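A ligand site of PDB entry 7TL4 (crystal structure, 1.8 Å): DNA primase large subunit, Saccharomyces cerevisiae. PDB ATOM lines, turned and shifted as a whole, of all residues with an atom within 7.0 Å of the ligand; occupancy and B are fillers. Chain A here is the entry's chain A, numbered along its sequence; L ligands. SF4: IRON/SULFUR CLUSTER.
OG1 of Thr 164 is in hydrogen-bond range of O of Thr 160 (2.8 Å). The side-chain sulfur of Cys 106 lies close to the backbone NH of His 188 (3.4 Å). SG of Cys 123 lies close to N of Phe 125, at 3.6 Å. O of Ala 187 sits at hydrogen-bond distance from N of Cys 106. SG of Cys 25 lies close to NE2 of Gln 46 (3.7 Å).
Residues that only touch the ligand: Pro 189 (3.5 Å), Phe 125 (3.6 Å), Pro 23 (3.7 Å), Thr 160 (3.9 Å) and Ile 109 (3.96 Å). Hydrophobic or aromatic side chains that line the ligand: Pro 23, Ile 109, Phe 125 and Pro 189. Within 4 Å of the ligand: Pro 23, Cys 25, Cys 106, Ile 109, Cys 123, Phe 125, Thr 160, Cys 163 and Pro 189.
SG of Cys 25 is bound to FE1 of the ligand, 2.4 Å away. The side-chain sulfur (SG) of Cys 106 is bound to an iron atom (FE2) of the ligand. The side-chain sulfur (SG) of Cys 123 binds an iron atom (FE4) of the ligand, 2.5 Å away. S2 of the ligand sits close to N of Cys 25. An iron atom (FE3) of the ligand is bound by the side-chain sulfur of Cys 163, at 2.4 Å.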
ATOM      1  N   PRO A  23      33.924 -10.275  -8.133  1.00  0.00           N
ATOM      2  CA  PRO A  23      32.759  -9.863  -7.325  1.00  0.00           C
ATOM      3  C   PRO A  23      31.497 -10.485  -7.930  1.00  0.00           C
ATOM      4  O   PRO A  23      31.510 -11.019  -9.021  1.00  0.00           O
ATOM      5  CB  PRO A  23      32.735  -8.329  -7.473  1.00  0.00           C
ATOM      6  CG  PRO A  23      33.383  -8.053  -8.824  1.00  0.00           C
ATOM      7  CD  PRO A  23      34.452  -9.165  -8.951  1.00  0.00           C
ATOM      8  N   LEU A  24      30.383 -10.400  -7.202  1.00  0.00           N
ATOM      9  CA  LEU A  24      29.204 -11.171  -7.624  1.00  0.00           C
ATOM     10  C   LEU A  24      28.731 -10.779  -9.031  1.00  0.00           C
ATOM     11  O   LEU A  24      28.219 -11.630  -9.769  1.00  0.00           O
ATOM     12  CB  LEU A  24      28.052 -11.002  -6.613  1.00  0.00           C
ATOM     13  CG  LEU A  24      28.100 -11.574  -5.198  1.00  0.00           C
ATOM     14  CD1 LEU A  24      26.700 -11.862  -4.621  1.00  0.00           C
ATOM     15  CD2 LEU A  24      28.941 -12.831  -5.129  1.00  0.00           C
ATOM     16  N   CYS A  25      28.818  -9.486  -9.412  1.00  0.00           N
ATOM     17  CA  CYS A  25      28.309  -9.118 -10.746  1.00  0.00           C
ATOM     18  C   CYS A  25      29.096  -9.833 -11.855  1.00  0.00           C
ATOM     19  O   CYS A  25      28.501 -10.382 -12.785  1.00  0.00           O
ATOM     20  CB  CYS A  25      28.383  -7.608 -11.047  1.00  0.00           C
ATOM     21  SG  CYS A  25      30.039  -6.880 -10.773  1.00  0.00           S
ATOM     22  N   ILE A  26      30.422  -9.860 -11.731  1.00  0.00           N
ATOM     23  CA  ILE A  26      31.249 -10.566 -12.727  1.00  0.00           C
ATOM     24  C   ILE A  26      30.986 -12.076 -12.666  1.00  0.00           C
ATOM     25  O   ILE A  26      30.969 -12.729 -13.699  1.00  0.00           O
ATOM     26  CB  ILE A  26      32.753 -10.252 -12.514  1.00  0.00           C
ATOM     27  CG1 ILE A  26      33.021  -8.740 -12.660  1.00  0.00           C
ATOM     28  CG2 ILE A  26      33.652 -11.045 -13.542  1.00  0.00           C
ATOM     29  CD1 ILE A  26      32.333  -8.036 -13.956  1.00  0.00           C
ATOM     30  N   GLN A  46      29.887  -4.849 -19.825  1.00  0.00           N
ATOM     31  CA  GLN A  46      30.345  -4.845 -18.456  1.00  0.00           C
ATOM     32  C   GLN A  46      31.441  -5.882 -18.251  1.00  0.00           C
ATOM     33  O   GLN A  46      32.484  -5.603 -17.621  1.00  0.00           O
ATOM     34  CB  GLN A  46      29.159  -5.129 -17.510  1.00  0.00           C
ATOM     35  CG  GLN A  46      29.456  -5.117 -15.960  1.00  0.00           C
ATOM     36  CD  GLN A  46      28.176  -5.194 -15.139  1.00  0.00           C
ATOM     37  OE1 GLN A  46      27.070  -4.935 -15.630  1.00  0.00           O
ATOM     38  NE2 GLN A  46      28.333  -5.569 -13.831  1.00  0.00           N
ATOM     39  N   ASP A 105      32.898   1.465 -13.298  1.00  0.00           N
ATOM     40  CA  ASP A 105      32.836   1.415 -11.827  1.00  0.00           C
ATOM     41  C   ASP A 105      31.419   1.091 -11.342  1.00  0.00           C
ATOM     42  O   ASP A 105      30.465   0.980 -12.140  1.00  0.00           O
ATOM     43  CB  ASP A 105      33.336   2.715 -11.194  1.00  0.00           C
ATOM     44  CG  ASP A 105      32.454   3.911 -11.514  1.00  0.00           C
ATOM     45  OD1 ASP A 105      31.419   3.778 -12.192  1.00  0.00           O
ATOM     46  OD2 ASP A 105      32.825   5.022 -11.075  1.00  0.00           O
ATOM     47  N   CYS A 106      31.275   0.985  -9.988  1.00  0.00           N
ATOM     48  CA  CYS A 106      30.006   0.510  -9.456  1.00  0.00           C
ATOM     49  C   CYS A 106      28.881   1.487  -9.810  1.00  0.00           C
ATOM     50  O   CYS A 106      27.781   1.065 -10.164  1.00  0.00           O
ATOM     51  CB  CYS A 106      30.077   0.291  -7.931  1.00  0.00           C
ATOM     52  SG  CYS A 106      31.258  -1.090  -7.565  1.00  0.00           S
ATOM     53  N   HIS A 107      29.151   2.770  -9.682  1.00  0.00           N
ATOM     54  CA  HIS A 107      28.128   3.785  -9.942  1.00  0.00           C
ATOM     55  C   HIS A 107      27.652   3.701 -11.389  1.00  0.00           C
ATOM     56  O   HIS A 107      26.451   3.858 -11.676  1.00  0.00           O
ATOM     57  CB  HIS A 107      28.707   5.130  -9.636  1.00  0.00           C
ATOM     58  CG  HIS A 107      27.791   6.284  -9.956  1.00  0.00           C
ATOM     59  ND1 HIS A 107      26.604   6.488  -9.287  1.00  0.00           N
ATOM     60  CD2 HIS A 107      27.926   7.309 -10.823  1.00  0.00           C
ATOM     61  CE1 HIS A 107      26.030   7.592  -9.756  1.00  0.00           C
ATOM     62  NE2 HIS A 107      26.814   8.112 -10.696  1.00  0.00           N
ATOM     63  N   ILE A 109      27.708   0.986 -13.373  1.00  0.00           N
ATOM     64  CA  ILE A 109      26.948  -0.253 -13.488  1.00  0.00           C
ATOM     65  C   ILE A 109      25.545  -0.075 -12.939  1.00  0.00           C
ATOM     66  O   ILE A 109      24.566  -0.528 -13.556  1.00  0.00           O
ATOM     67  CB  ILE A 109      27.693  -1.384 -12.752  1.00  0.00           C
ATOM     68  CG1 ILE A 109      28.893  -1.846 -13.597  1.00  0.00           C
ATOM     69  CG2 ILE A 109      26.748  -2.548 -12.612  1.00  0.00           C
ATOM     70  CD1 ILE A 109      29.975  -2.593 -12.732  1.00  0.00           C
ATOM     71  N   LEU A 110      25.421   0.531 -11.745  1.00  0.00           N
ATOM     72  CA  LEU A 110      24.119   0.705 -11.121  1.00  0.00           C
ATOM     73  C   LEU A 110      23.264   1.682 -11.927  1.00  0.00           C
ATOM     74  O   LEU A 110      22.032   1.657 -11.837  1.00  0.00           O
ATOM     75  CB  LEU A 110      24.260   1.213  -9.683  1.00  0.00           C
ATOM     76  CG  LEU A 110      24.909   0.168  -8.709  1.00  0.00           C
ATOM     77  CD1 LEU A 110      25.327   1.023  -7.523  1.00  0.00           C
ATOM     78  CD2 LEU A 110      23.873  -0.828  -8.259  1.00  0.00           C
ATOM     79  N   GLY A 122      24.411  -5.386 -14.405  1.00  0.00           N
ATOM     80  CA  GLY A 122      23.885  -4.756 -13.162  1.00  0.00           C
ATOM     81  C   GLY A 122      24.628  -5.238 -11.942  1.00  0.00           C
ATOM     82  O   GLY A 122      25.765  -5.707 -12.033  1.00  0.00           O
ATOM     83  N   CYS A 123      23.946  -5.150 -10.787  1.00  0.00           N
ATOM     84  CA  CYS A 123      24.537  -5.470  -9.487  1.00  0.00           C
ATOM     85  C   CYS A 123      23.653  -6.466  -8.768  1.00  0.00           C
ATOM     86  O   CYS A 123      22.485  -6.143  -8.465  1.00  0.00           O
ATOM     87  CB  CYS A 123      24.714  -4.192  -8.661  1.00  0.00           C
ATOM     88  SG  CYS A 123      25.225  -4.574  -6.968  1.00  0.00           S
ATOM     89  N   PRO A 124      24.143  -7.703  -8.510  1.00  0.00           N
ATOM     90  CA  PRO A 124      23.277  -8.707  -7.891  1.00  0.00           C
ATOM     91  C   PRO A 124      22.756  -8.321  -6.557  1.00  0.00           C
ATOM     92  O   PRO A 124      21.656  -8.785  -6.194  1.00  0.00           O
ATOM     93  CB  PRO A 124      24.196  -9.940  -7.771  1.00  0.00           C
ATOM     94  CG  PRO A 124      25.060  -9.819  -9.013  1.00  0.00           C
ATOM     95  CD  PRO A 124      25.330  -8.329  -9.157  1.00  0.00           C
ATOM     96  N   PHE A 125      23.487  -7.484  -5.803  1.00  0.00           N
ATOM     97  CA  PHE A 125      23.001  -7.084  -4.488  1.00  0.00           C
ATOM     98  C   PHE A 125      21.720  -6.264  -4.583  1.00  0.00           C
ATOM     99  O   PHE A 125      20.907  -6.283  -3.661  1.00  0.00           O
ATOM    100  CB  PHE A 125      24.110  -6.280  -3.772  1.00  0.00           C
ATOM    101  CG  PHE A 125      25.306  -7.119  -3.450  1.00  0.00           C
ATOM    102  CD1 PHE A 125      25.195  -8.111  -2.435  1.00  0.00           C
ATOM    103  CD2 PHE A 125      26.503  -6.984  -4.156  1.00  0.00           C
ATOM    104  CE1 PHE A 125      26.255  -8.948  -2.126  1.00  0.00           C
ATOM    105  CE2 PHE A 125      27.586  -7.809  -3.893  1.00  0.00           C
ATOM    106  CZ  PHE A 125      27.491  -8.778  -2.829  1.00  0.00           C
ATOM    107  N   ARG A 126      21.542  -5.494  -5.673  1.00  0.00           N
ATOM    108  CA  ARG A 126      20.267  -4.848  -5.973  1.00  0.00           C
ATOM    109  C   ARG A 126      19.311  -5.758  -6.739  1.00  0.00           C
ATOM    110  O   ARG A 126      18.104  -5.751  -6.468  1.00  0.00           O
ATOM    111  CB  ARG A 126      20.497  -3.568  -6.847  1.00  0.00           C
ATOM    112  CG  ARG A 126      19.205  -2.857  -7.255  1.00  0.00           C
ATOM    113  CD  ARG A 126      19.463  -1.816  -8.310  1.00  0.00           C
ATOM    114  NE  ARG A 126      19.946  -2.445  -9.506  1.00  0.00           N
ATOM    115  CZ  ARG A 126      20.537  -1.792 -10.511  1.00  0.00           C
ATOM    116  NH1 ARG A 126      20.649  -0.449 -10.440  1.00  0.00           N
ATOM    117  NH2 ARG A 126      20.985  -2.491 -11.555  1.00  0.00           N
ATOM    118  N   TYR A 159      24.355  -1.068  -1.713  1.00  0.00           N
ATOM    119  CA  TYR A 159      24.867  -2.244  -2.435  1.00  0.00           C
ATOM    120  C   TYR A 159      26.380  -2.340  -2.348  1.00  0.00           C
ATOM    121  O   TYR A 159      26.920  -3.454  -2.173  1.00  0.00           O
ATOM    122  CB  TYR A 159      24.383  -2.225  -3.880  1.00  0.00           C
ATOM    123  CG  TYR A 159      22.891  -2.005  -3.910  1.00  0.00           C
ATOM    124  CD1 TYR A 159      22.049  -2.885  -3.278  1.00  0.00           C
ATOM    125  CD2 TYR A 159      22.348  -0.889  -4.519  1.00  0.00           C
ATOM    126  CE1 TYR A 159      20.674  -2.670  -3.271  1.00  0.00           C
ATOM    127  CE2 TYR A 159      21.002  -0.681  -4.511  1.00  0.00           C
ATOM    128  CZ  TYR A 159      20.159  -1.573  -3.922  1.00  0.00           C
ATOM    129  OH  TYR A 159      18.798  -1.320  -3.889  1.00  0.00           O
ATOM    130  N   THR A 160      27.097  -1.227  -2.460  1.00  0.00           N
ATOM    131  CA  THR A 160      28.561  -1.361  -2.445  1.00  0.00           C
ATOM    132  C   THR A 160      29.053  -1.728  -1.032  1.00  0.00           C
ATOM    133  O   THR A 160      30.107  -2.384  -0.865  1.00  0.00           O
ATOM    134  CB  THR A 160      29.239  -0.073  -2.940  1.00  0.00           C
ATOM    135  OG1 THR A 160      28.854   0.997  -2.096  1.00  0.00           O
ATOM    136  CG2 THR A 160      28.822   0.265  -4.397  1.00  0.00           C
ATOM    137  N   ILE A 161      28.291  -1.392  -0.010  1.00  0.00           N
ATOM    138  CA  ILE A 161      28.635  -1.854   1.326  1.00  0.00           C
ATOM    139  C   ILE A 161      28.410  -3.346   1.455  1.00  0.00           C
ATOM    140  O   ILE A 161      29.207  -4.063   2.082  1.00  0.00           O
ATOM    141  CB  ILE A 161      27.821  -1.088   2.379  1.00  0.00           C
ATOM    142  CG1 ILE A 161      28.136   0.389   2.308  1.00  0.00           C
ATOM    143  CG2 ILE A 161      28.091  -1.608   3.785  1.00  0.00           C
ATOM    144  CD1 ILE A 161      29.508   0.720   2.877  1.00  0.00           C
ATOM    145  N   ALA A 162      27.307  -3.831   0.887  1.00  0.00           N
ATOM    146  CA  ALA A 162      27.056  -5.278   0.938  1.00  0.00           C
ATOM    147  C   ALA A 162      28.165  -6.050   0.224  1.00  0.00           C
ATOM    148  O   ALA A 162      28.612  -7.105   0.704  1.00  0.00           O
ATOM    149  CB  ALA A 162      25.704  -5.581   0.300  1.00  0.00           C
ATOM    150  N   CYS A 163      28.648  -5.493  -0.896  1.00  0.00           N
ATOM    151  CA  CYS A 163      29.735  -6.100  -1.650  1.00  0.00           C
ATOM    152  C   CYS A 163      31.019  -6.115  -0.828  1.00  0.00           C
ATOM    153  O   CYS A 163      31.729  -7.139  -0.762  1.00  0.00           O
ATOM    154  CB  CYS A 163      29.897  -5.318  -2.958  1.00  0.00           C
ATOM    155  SG  CYS A 163      31.049  -6.106  -4.097  1.00  0.00           S
ATOM    156  N   THR A 164      31.311  -4.979  -0.185  1.00  0.00           N
ATOM    157  CA  THR A 164      32.464  -4.908   0.697  1.00  0.00           C
ATOM    158  C   THR A 164      32.343  -5.946   1.819  1.00  0.00           C
ATOM    159  O   THR A 164      33.327  -6.615   2.163  1.00  0.00           O
ATOM    160  CB  THR A 164      32.565  -3.503   1.290  1.00  0.00           C
ATOM    161  OG1 THR A 164      32.685  -2.532   0.225  1.00  0.00           O
ATOM    162  CG2 THR A 164      33.781  -3.407   2.262  1.00  0.00           C
ATOM    163  N   ALA A 187      34.352   2.723  -5.373  1.00  0.00           N
ATOM    164  CA  ALA A 187      33.645   1.452  -5.541  1.00  0.00           C
ATOM    165  C   ALA A 187      33.826   1.017  -6.991  1.00  0.00           C
ATOM    166  O   ALA A 187      33.334   1.684  -7.901  1.00  0.00           O
ATOM    167  CB  ALA A 187      32.170   1.560  -5.212  1.00  0.00           C
ATOM    168  N   HIS A 188      34.489  -0.125  -7.197  1.00  0.00           N
ATOM    169  CA  HIS A 188      34.879  -0.517  -8.542  1.00  0.00           C
ATOM    170  C   HIS A 188      35.135  -2.008  -8.583  1.00  0.00           C
ATOM    171  O   HIS A 188      35.949  -2.489  -7.788  1.00  0.00           O
ATOM    172  CB  HIS A 188      36.125   0.258  -8.981  1.00  0.00           C
ATOM    173  CG  HIS A 188      36.317   0.315 -10.475  1.00  0.00           C
ATOM    174  ND1 HIS A 188      36.409  -0.808 -11.253  1.00  0.00           N
ATOM    175  CD2 HIS A 188      36.434   1.372 -11.318  1.00  0.00           C
ATOM    176  CE1 HIS A 188      36.551  -0.465 -12.523  1.00  0.00           C
ATOM    177  NE2 HIS A 188      36.598   0.861 -12.587  1.00  0.00           N
ATOM    178  N   PRO A 189      34.420  -2.766  -9.421  1.00  0.00           N
ATOM    179  CA  PRO A 189      34.697  -4.208  -9.574  1.00  0.00           C
ATOM    180  C   PRO A 189      36.177  -4.577  -9.747  1.00  0.00           C
ATOM    181  O   PRO A 189      36.625  -5.618  -9.224  1.00  0.00           O
ATOM    182  CB  PRO A 189      33.893  -4.581 -10.838  1.00  0.00           C
ATOM    183  CG  PRO A 189      32.750  -3.503 -10.891  1.00  0.00           C
ATOM    184  CD  PRO A 189      33.468  -2.253 -10.447  1.00  0.00           C
ATOM    185  N   ASN A 190      36.922  -3.806 -10.565  1.00  0.00           N
ATOM    186  CA  ASN A 190      38.346  -4.090 -10.743  1.00  0.00           C
ATOM    187  C   ASN A 190      39.129  -3.865  -9.458  1.00  0.00           C
ATOM    188  O   ASN A 190      40.160  -4.518  -9.236  1.00  0.00           O
ATOM    189  CB  ASN A 190      38.904  -3.216 -11.860  1.00  0.00           C
ATOM    190  CG  ASN A 190      38.422  -3.678 -13.246  1.00  0.00           C
ATOM    191  OD1 ASN A 190      37.331  -3.265 -13.685  1.00  0.00           O
ATOM    192  ND2 ASN A 190      39.182  -4.571 -13.891  1.00  0.00           N
ATOM    193  N   TYR A 192      37.881  -4.553  -6.502  1.00  0.00           N
ATOM    194  CA  TYR A 192      37.601  -5.801  -5.791  1.00  0.00           C
ATOM    195  C   TYR A 192      38.534  -6.905  -6.278  1.00  0.00           C
ATOM    196  O   TYR A 192      39.152  -7.611  -5.466  1.00  0.00           O
ATOM    197  CB  TYR A 192      36.149  -6.227  -6.041  1.00  0.00           C
ATOM    198  CG  TYR A 192      35.548  -7.365  -5.176  1.00  0.00           C
ATOM    199  CD1 TYR A 192      35.929  -8.690  -5.380  1.00  0.00           C
ATOM    200  CD2 TYR A 192      34.493  -7.088  -4.315  1.00  0.00           C
ATOM    201  CE1 TYR A 192      35.345  -9.746  -4.675  1.00  0.00           C
ATOM    202  CE2 TYR A 192      33.911  -8.109  -3.579  1.00  0.00           C
ATOM    203  CZ  TYR A 192      34.314  -9.426  -3.753  1.00  0.00           C
ATOM    204  OH  TYR A 192      33.681 -10.385  -3.030  1.00  0.00           O
HETATM  205 FE1  SF4 L   1      29.740  -5.546  -8.814  1.00  0.00          FE
HETATM  206 FE2  SF4 L   1      29.982  -3.116  -7.580  1.00  0.00          FE
HETATM  207 FE3  SF4 L   1      30.095  -5.393  -6.153  1.00  0.00          FE
HETATM  208 FE4  SF4 L   1      27.746  -4.635  -7.270  1.00  0.00          FE
HETATM  209  S1  SF4 L   1      28.844  -3.491  -5.689  1.00  0.00           S
HETATM  210  S2  SF4 L   1      28.650  -6.735  -7.162  1.00  0.00           S
HETATM  211  S3  SF4 L   1      28.451  -3.654  -9.209  1.00  0.00           S
HETATM  212  S4  SF4 L   1      31.569  -4.805  -7.809  1.00  0.00           S
